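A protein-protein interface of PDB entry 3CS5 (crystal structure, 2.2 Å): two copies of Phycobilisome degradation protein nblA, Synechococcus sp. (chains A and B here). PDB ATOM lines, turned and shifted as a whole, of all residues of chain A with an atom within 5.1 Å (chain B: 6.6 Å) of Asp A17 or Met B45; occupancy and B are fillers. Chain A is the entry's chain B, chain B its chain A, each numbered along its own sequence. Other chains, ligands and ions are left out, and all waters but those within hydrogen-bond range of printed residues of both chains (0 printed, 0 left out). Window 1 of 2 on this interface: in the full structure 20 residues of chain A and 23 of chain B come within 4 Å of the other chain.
OD2 of Asp A17 lies within hydrogen-bond range of OH of Tyr A21 (3.3 Å).
Among the printed residues, pairs that only touch across the chains: Leu A18 with Val B41 (3.1 Å), Leu A18 with Arg B42 (3.2 Å), Tyr A21 with Val B41 (3.3 Å), Gln A14 with Met B45 (3.5 Å), Gln A14 with Asn B49 (3.6 Å) and Asp A17 with Met B45 (3.9 Å).
Of chain B, only Met B45 (3.9 Å) comes within 4 Å of Asp A17.
Met B45 touches two residues of chain A.
Printed residues of chain A within 4 Å of Arg B42: Leu A18.
Printed residues of chain B within 4 Å of Tyr A21: Val B41.
Of the printed residues of chain A, Asn B49 touches Gln A14.
Printed residues of chain A within 4 Å of Val B41: Leu A18 (3.1 Å) and Tyr A21 (3.3 Å).
Of the printed residues of chain B, Leu A18 touches Val B41 (3.1 Å) and Arg B42 (3.2 Å).
His B47 touches none of the printed residues of chain A.
The nearest residue of chain A that does not touch Met B45 is Leu A18 (4.2 Å).
The nearest printed residue of chain B that does not touch Gln A14 is Glu B48 (4.2 Å).
Hydrophobic or aromatic side chains of chain B within 4 Å of the printed part of chain A: Val B41 and Met B45.
Printed residues of chain A that touch a printed residue of chain B: Gln A14, Asp A17, Leu A18 and Tyr A21.
Hydrophobic or aromatic side chains of chain A within 4 Å of the printed part of chain B: Leu A18 and Tyr A21.
Along chain A the printed residues that touch a printed residue of chain B span positions 14 to 21.
Among the printed residues, no Asp or Glu carboxylate lies within 4 Å of a Lys or Arg side-chain nitrogen of the other chain.
No position is printed for both chains.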
ATOM      1  N   GLU A  13      -5.096 -12.232 -19.243  1.00  0.00           N
ATOM      2  CA  GLU A  13      -4.621 -11.437 -20.366  1.00  0.00           C
ATOM      3  C   GLU A  13      -5.487 -10.203 -20.614  1.00  0.00           C
ATOM      4  O   GLU A  13      -4.945  -9.148 -20.960  1.00  0.00           O
ATOM      5  CB  GLU A  13      -4.573 -12.304 -21.629  1.00  0.00           C
ATOM      6  CG  GLU A  13      -4.363 -11.561 -22.940  1.00  0.00           C
ATOM      7  CD  GLU A  13      -4.378 -12.545 -24.101  1.00  0.00           C
ATOM      8  OE1 GLU A  13      -5.401 -12.641 -24.800  1.00  0.00           O
ATOM      9  OE2 GLU A  13      -3.366 -13.241 -24.318  1.00  0.00           O
ATOM     10  N   GLN A  14      -6.793 -10.375 -20.441  1.00  0.00           N
ATOM     11  CA  GLN A  14      -7.784  -9.324 -20.629  1.00  0.00           C
ATOM     12  C   GLN A  14      -7.498  -8.183 -19.645  1.00  0.00           C
ATOM     13  O   GLN A  14      -7.334  -7.041 -20.086  1.00  0.00           O
ATOM     14  CB  GLN A  14      -9.213  -9.815 -20.443  1.00  0.00           C
ATOM     15  CG  GLN A  14      -9.616 -11.100 -21.148  1.00  0.00           C
ATOM     16  CD  GLN A  14     -11.095 -11.129 -21.502  1.00  0.00           C
ATOM     17  OE1 GLN A  14     -11.973 -11.222 -20.648  1.00  0.00           O
ATOM     18  NE2 GLN A  14     -11.403 -11.047 -22.800  1.00  0.00           N
ATOM     19  N   GLN A  15      -7.445  -8.556 -18.369  1.00  0.00           N
ATOM     20  CA  GLN A  15      -7.111  -7.644 -17.279  1.00  0.00           C
ATOM     21  C   GLN A  15      -5.886  -6.810 -17.685  1.00  0.00           C
ATOM     22  O   GLN A  15      -5.964  -5.601 -17.533  1.00  0.00           O
ATOM     23  CB  GLN A  15      -6.812  -8.338 -15.955  1.00  0.00           C
ATOM     24  CG  GLN A  15      -7.784  -9.410 -15.510  1.00  0.00           C
ATOM     25  CD  GLN A  15      -7.572  -9.840 -14.073  1.00  0.00           C
ATOM     26  OE1 GLN A  15      -6.832  -9.207 -13.315  1.00  0.00           O
ATOM     27  NE2 GLN A  15      -8.218 -10.930 -13.671  1.00  0.00           N
ATOM     28  N   PHE A  16      -4.864  -7.497 -18.172  1.00  0.00           N
ATOM     29  CA  PHE A  16      -3.622  -6.973 -18.714  1.00  0.00           C
ATOM     30  C   PHE A  16      -3.921  -5.898 -19.764  1.00  0.00           C
ATOM     31  O   PHE A  16      -3.382  -4.796 -19.697  1.00  0.00           O
ATOM     32  CB  PHE A  16      -2.744  -8.064 -19.338  1.00  0.00           C
ATOM     33  CG  PHE A  16      -2.026  -8.972 -18.348  1.00  0.00           C
ATOM     34  CD1 PHE A  16      -2.420 -10.289 -18.171  1.00  0.00           C
ATOM     35  CD2 PHE A  16      -0.961  -8.523 -17.585  1.00  0.00           C
ATOM     36  CE1 PHE A  16      -1.792 -11.135 -17.276  1.00  0.00           C
ATOM     37  CE2 PHE A  16      -0.320  -9.355 -16.686  1.00  0.00           C
ATOM     38  CZ  PHE A  16      -0.725 -10.667 -16.515  1.00  0.00           C
ATOM     39  N   ASP A  17      -4.779  -6.247 -20.709  1.00  0.00           N
ATOM     40  CA  ASP A  17      -5.188  -5.387 -21.813  1.00  0.00           C
ATOM     41  C   ASP A  17      -5.777  -4.076 -21.304  1.00  0.00           C
ATOM     42  O   ASP A  17      -5.203  -3.014 -21.566  1.00  0.00           O
ATOM     43  CB  ASP A  17      -6.198  -6.118 -22.694  1.00  0.00           C
ATOM     44  CG  ASP A  17      -5.777  -6.256 -24.141  1.00  0.00           C
ATOM     45  OD1 ASP A  17      -4.606  -6.610 -24.398  1.00  0.00           O
ATOM     46  OD2 ASP A  17      -6.625  -6.000 -25.027  1.00  0.00           O
ATOM     47  N   LEU A  18      -6.892  -4.169 -20.590  1.00  0.00           N
ATOM     48  CA  LEU A  18      -7.648  -3.025 -20.106  1.00  0.00           C
ATOM     49  C   LEU A  18      -6.731  -1.963 -19.489  1.00  0.00           C
ATOM     50  O   LEU A  18      -6.951  -0.771 -19.691  1.00  0.00           O
ATOM     51  CB  LEU A  18      -8.701  -3.440 -19.076  1.00  0.00           C
ATOM     52  CG  LEU A  18      -9.132  -4.901 -19.059  1.00  0.00           C
ATOM     53  CD1 LEU A  18     -10.010  -5.188 -17.845  1.00  0.00           C
ATOM     54  CD2 LEU A  18      -9.858  -5.259 -20.348  1.00  0.00           C
ATOM     55  N   GLN A  19      -5.731  -2.458 -18.784  1.00  0.00           N
ATOM     56  CA  GLN A  19      -4.660  -1.739 -18.129  1.00  0.00           C
ATOM     57  C   GLN A  19      -3.752  -1.018 -19.122  1.00  0.00           C
ATOM     58  O   GLN A  19      -3.260   0.087 -18.869  1.00  0.00           O
ATOM     59  CB  GLN A  19      -3.840  -2.735 -17.310  1.00  0.00           C
ATOM     60  CG  GLN A  19      -4.272  -2.971 -15.874  1.00  0.00           C
ATOM     61  CD  GLN A  19      -3.396  -4.024 -15.217  1.00  0.00           C
ATOM     62  OE1 GLN A  19      -2.217  -4.157 -15.553  1.00  0.00           O
ATOM     63  NE2 GLN A  19      -3.951  -4.787 -14.278  1.00  0.00           N
ATOM     64  N   LYS A  20      -3.501  -1.641 -20.280  1.00  0.00           N
ATOM     65  CA  LYS A  20      -2.677  -0.960 -21.280  1.00  0.00           C
ATOM     66  C   LYS A  20      -3.475   0.137 -21.975  1.00  0.00           C
ATOM     67  O   LYS A  20      -2.942   1.042 -22.607  1.00  0.00           O
ATOM     68  CB  LYS A  20      -2.142  -1.959 -22.304  1.00  0.00           C
ATOM     69  CG  LYS A  20      -2.416  -3.412 -21.932  1.00  0.00           C
ATOM     70  CD  LYS A  20      -2.381  -4.310 -23.160  1.00  0.00           C
ATOM     71  CE  LYS A  20      -1.405  -5.466 -22.970  1.00  0.00           C
ATOM     72  NZ  LYS A  20      -0.295  -5.417 -23.966  1.00  0.00           N
ATOM     73  N   TYR A  21      -4.794   0.043 -21.846  1.00  0.00           N
ATOM     74  CA  TYR A  21      -5.694   1.016 -22.453  1.00  0.00           C
ATOM     75  C   TYR A  21      -5.975   2.175 -21.503  1.00  0.00           C
ATOM     76  O   TYR A  21      -6.290   3.284 -21.937  1.00  0.00           O
ATOM     77  CB  TYR A  21      -7.006   0.346 -22.867  1.00  0.00           C
ATOM     78  CG  TYR A  21      -6.856  -0.652 -23.992  1.00  0.00           C
ATOM     79  CD1 TYR A  21      -5.881  -1.639 -23.945  1.00  0.00           C
ATOM     80  CD2 TYR A  21      -7.690  -0.608 -25.102  1.00  0.00           C
ATOM     81  CE1 TYR A  21      -5.739  -2.555 -24.971  1.00  0.00           C
ATOM     82  CE2 TYR A  21      -7.556  -1.519 -26.133  1.00  0.00           C
ATOM     83  CZ  TYR A  21      -6.580  -2.489 -26.063  1.00  0.00           C
ATOM     84  OH  TYR A  21      -6.443  -3.397 -27.087  1.00  0.00           O
ATOM     85  N   VAL B  40     -15.361   0.270 -20.715  1.00  0.00           N
ATOM     86  CA  VAL B  40     -15.789  -0.189 -22.019  1.00  0.00           C
ATOM     87  C   VAL B  40     -14.944  -1.301 -22.619  1.00  0.00           C
ATOM     88  O   VAL B  40     -15.411  -2.376 -23.001  1.00  0.00           O
ATOM     89  CB  VAL B  40     -15.718   1.002 -23.011  1.00  0.00           C
ATOM     90  CG1 VAL B  40     -15.607   0.398 -24.408  1.00  0.00           C
ATOM     91  CG2 VAL B  40     -16.957   1.866 -22.711  1.00  0.00           C
ATOM     92  N   VAL B  41     -13.639  -1.035 -22.669  1.00  0.00           N
ATOM     93  CA  VAL B  41     -12.668  -2.032 -23.104  1.00  0.00           C
ATOM     94  C   VAL B  41     -12.571  -3.164 -22.084  1.00  0.00           C
ATOM     95  O   VAL B  41     -11.946  -4.175 -22.397  1.00  0.00           O
ATOM     96  CB  VAL B  41     -11.271  -1.432 -23.339  1.00  0.00           C
ATOM     97  CG1 VAL B  41     -10.581  -2.172 -24.481  1.00  0.00           C
ATOM     98  CG2 VAL B  41     -11.394   0.058 -23.631  1.00  0.00           C
ATOM     99  N   ARG B  42     -13.170  -2.995 -20.910  1.00  0.00           N
ATOM    100  CA  ARG B  42     -13.672  -4.124 -20.136  1.00  0.00           C
ATOM    101  C   ARG B  42     -14.957  -4.679 -20.742  1.00  0.00           C
ATOM    102  O   ARG B  42     -15.080  -5.885 -20.961  1.00  0.00           O
ATOM    103  CB  ARG B  42     -13.912  -3.713 -18.682  1.00  0.00           C
ATOM    104  CG  ARG B  42     -12.650  -3.317 -17.933  1.00  0.00           C
ATOM    105  CD  ARG B  42     -12.943  -3.033 -16.469  1.00  0.00           C
ATOM    106  NE  ARG B  42     -11.784  -2.479 -15.776  1.00  0.00           N
ATOM    107  CZ  ARG B  42     -11.149  -1.373 -16.149  1.00  0.00           C
ATOM    108  NH1 ARG B  42     -11.291  -0.255 -15.447  1.00  0.00           N
ATOM    109  NH2 ARG B  42     -10.372  -1.382 -17.222  1.00  0.00           N
ATOM    110  N   GLN B  43     -15.910  -3.793 -21.010  1.00  0.00           N
ATOM    111  CA  GLN B  43     -17.190  -4.192 -21.581  1.00  0.00           C
ATOM    112  C   GLN B  43     -16.998  -5.192 -22.723  1.00  0.00           C
ATOM    113  O   GLN B  43     -17.147  -6.395 -22.537  1.00  0.00           O
ATOM    114  CB  GLN B  43     -17.982  -2.982 -22.078  1.00  0.00           C
ATOM    115  CG  GLN B  43     -19.296  -2.724 -21.365  1.00  0.00           C
ATOM    116  CD  GLN B  43     -19.559  -1.252 -21.110  1.00  0.00           C
ATOM    117  OE1 GLN B  43     -19.560  -0.436 -22.035  1.00  0.00           O
ATOM    118  NE2 GLN B  43     -19.780  -0.895 -19.848  1.00  0.00           N
ATOM    119  N   LYS B  44     -16.675  -4.649 -23.886  1.00  0.00           N
ATOM    120  CA  LYS B  44     -16.410  -5.335 -25.133  1.00  0.00           C
ATOM    121  C   LYS B  44     -15.793  -6.720 -24.937  1.00  0.00           C
ATOM    122  O   LYS B  44     -16.213  -7.690 -25.573  1.00  0.00           O
ATOM    123  CB  LYS B  44     -15.489  -4.463 -26.003  1.00  0.00           C
ATOM    124  CG  LYS B  44     -15.609  -2.975 -25.709  1.00  0.00           C
ATOM    125  CD  LYS B  44     -14.327  -2.206 -25.942  1.00  0.00           C
ATOM    126  CE  LYS B  44     -14.444  -1.147 -27.041  1.00  0.00           C
ATOM    127  NZ  LYS B  44     -13.240  -1.149 -27.930  1.00  0.00           N
ATOM    128  N   MET B  45     -14.802  -6.829 -24.057  1.00  0.00           N
ATOM    129  CA  MET B  45     -14.084  -8.085 -23.855  1.00  0.00           C
ATOM    130  C   MET B  45     -14.965  -9.145 -23.208  1.00  0.00           C
ATOM    131  O   MET B  45     -14.872 -10.320 -23.582  1.00  0.00           O
ATOM    132  CB  MET B  45     -12.815  -7.835 -23.032  1.00  0.00           C
ATOM    133  CG  MET B  45     -11.859  -6.869 -23.724  1.00  0.00           C
ATOM    134  SD  MET B  45     -11.607  -7.275 -25.470  1.00  0.00           S
ATOM    135  CE  MET B  45      -9.965  -7.999 -25.387  1.00  0.00           C
ATOM    136  N   ALA B  46     -15.811  -8.720 -22.280  1.00  0.00           N
ATOM    137  CA  ALA B  46     -16.824  -9.539 -21.632  1.00  0.00           C
ATOM    138  C   ALA B  46     -17.712 -10.237 -22.663  1.00  0.00           C
ATOM    139  O   ALA B  46     -18.229 -11.340 -22.456  1.00  0.00           O
ATOM    140  CB  ALA B  46     -17.687  -8.698 -20.705  1.00  0.00           C
ATOM    141  N   HIS B  47     -17.870  -9.560 -23.792  1.00  0.00           N
ATOM    142  CA  HIS B  47     -18.531 -10.115 -24.958  1.00  0.00           C
ATOM    143  C   HIS B  47     -17.542 -11.010 -25.717  1.00  0.00           C
ATOM    144  O   HIS B  47     -17.953 -12.013 -26.292  1.00  0.00           O
ATOM    145  CB  HIS B  47     -19.054  -9.050 -25.909  1.00  0.00           C
ATOM    146  CG  HIS B  47     -19.914  -7.966 -25.355  1.00  0.00           C
ATOM    147  ND1 HIS B  47     -19.477  -7.034 -24.443  1.00  0.00           N
ATOM    148  CD2 HIS B  47     -21.213  -7.650 -25.601  1.00  0.00           C
ATOM    149  CE1 HIS B  47     -20.461  -6.200 -24.146  1.00  0.00           C
ATOM    150  NE2 HIS B  47     -21.523  -6.558 -24.842  1.00  0.00           N
ATOM    151  N   GLU B  48     -16.266 -10.616 -25.712  1.00  0.00           N
ATOM    152  CA  GLU B  48     -15.249 -11.364 -26.448  1.00  0.00           C
ATOM    153  C   GLU B  48     -15.305 -12.845 -26.070  1.00  0.00           C
ATOM    154  O   GLU B  48     -15.353 -13.713 -26.941  1.00  0.00           O
ATOM    155  CB  GLU B  48     -13.852 -10.792 -26.209  1.00  0.00           C
ATOM    156  CG  GLU B  48     -13.522  -9.569 -27.053  1.00  0.00           C
ATOM    157  CD  GLU B  48     -12.126  -9.565 -27.631  1.00  0.00           C
ATOM    158  OE1 GLU B  48     -11.237 -10.277 -27.116  1.00  0.00           O
ATOM    159  OE2 GLU B  48     -11.882  -8.819 -28.608  1.00  0.00           O
ATOM    160  N   ASN B  49     -15.324 -13.088 -24.772  1.00  0.00           N
ATOM    161  CA  ASN B  49     -15.523 -14.344 -24.087  1.00  0.00           C
ATOM    162  C   ASN B  49     -16.934 -14.884 -24.266  1.00  0.00           C
ATOM    163  O   ASN B  49     -17.268 -16.005 -23.893  1.00  0.00           O
ATOM    164  CB  ASN B  49     -15.300 -14.183 -22.575  1.00  0.00           C
ATOM    165  CG  ASN B  49     -13.914 -14.651 -22.181  1.00  0.00           C
ATOM    166  OD1 ASN B  49     -12.957 -14.301 -22.871  1.00  0.00           O
ATOM    167  ND2 ASN B  49     -13.825 -15.424 -21.110  1.00  0.00           N
ATOM    168  N   ILE B  50     -17.768 -14.022 -24.834  1.00  0.00           N
ATOM    169  CA  ILE B  50     -19.188 -14.302 -24.945  1.00  0.00           C
ATOM    170  C   ILE B  50     -19.513 -14.760 -26.362  1.00  0.00           C
ATOM    171  O   ILE B  50     -20.163 -15.790 -26.556  1.00  0.00           O
ATOM    172  CB  ILE B  50     -19.968 -13.034 -24.522  1.00  0.00           C
ATOM    173  CG1 ILE B  50     -20.356 -13.090 -23.023  1.00  0.00           C
ATOM    174  CG2 ILE B  50     -21.178 -12.789 -25.435  1.00  0.00           C
ATOM    175  CD1 ILE B  50     -20.058 -14.445 -22.397  1.00  0.00           C
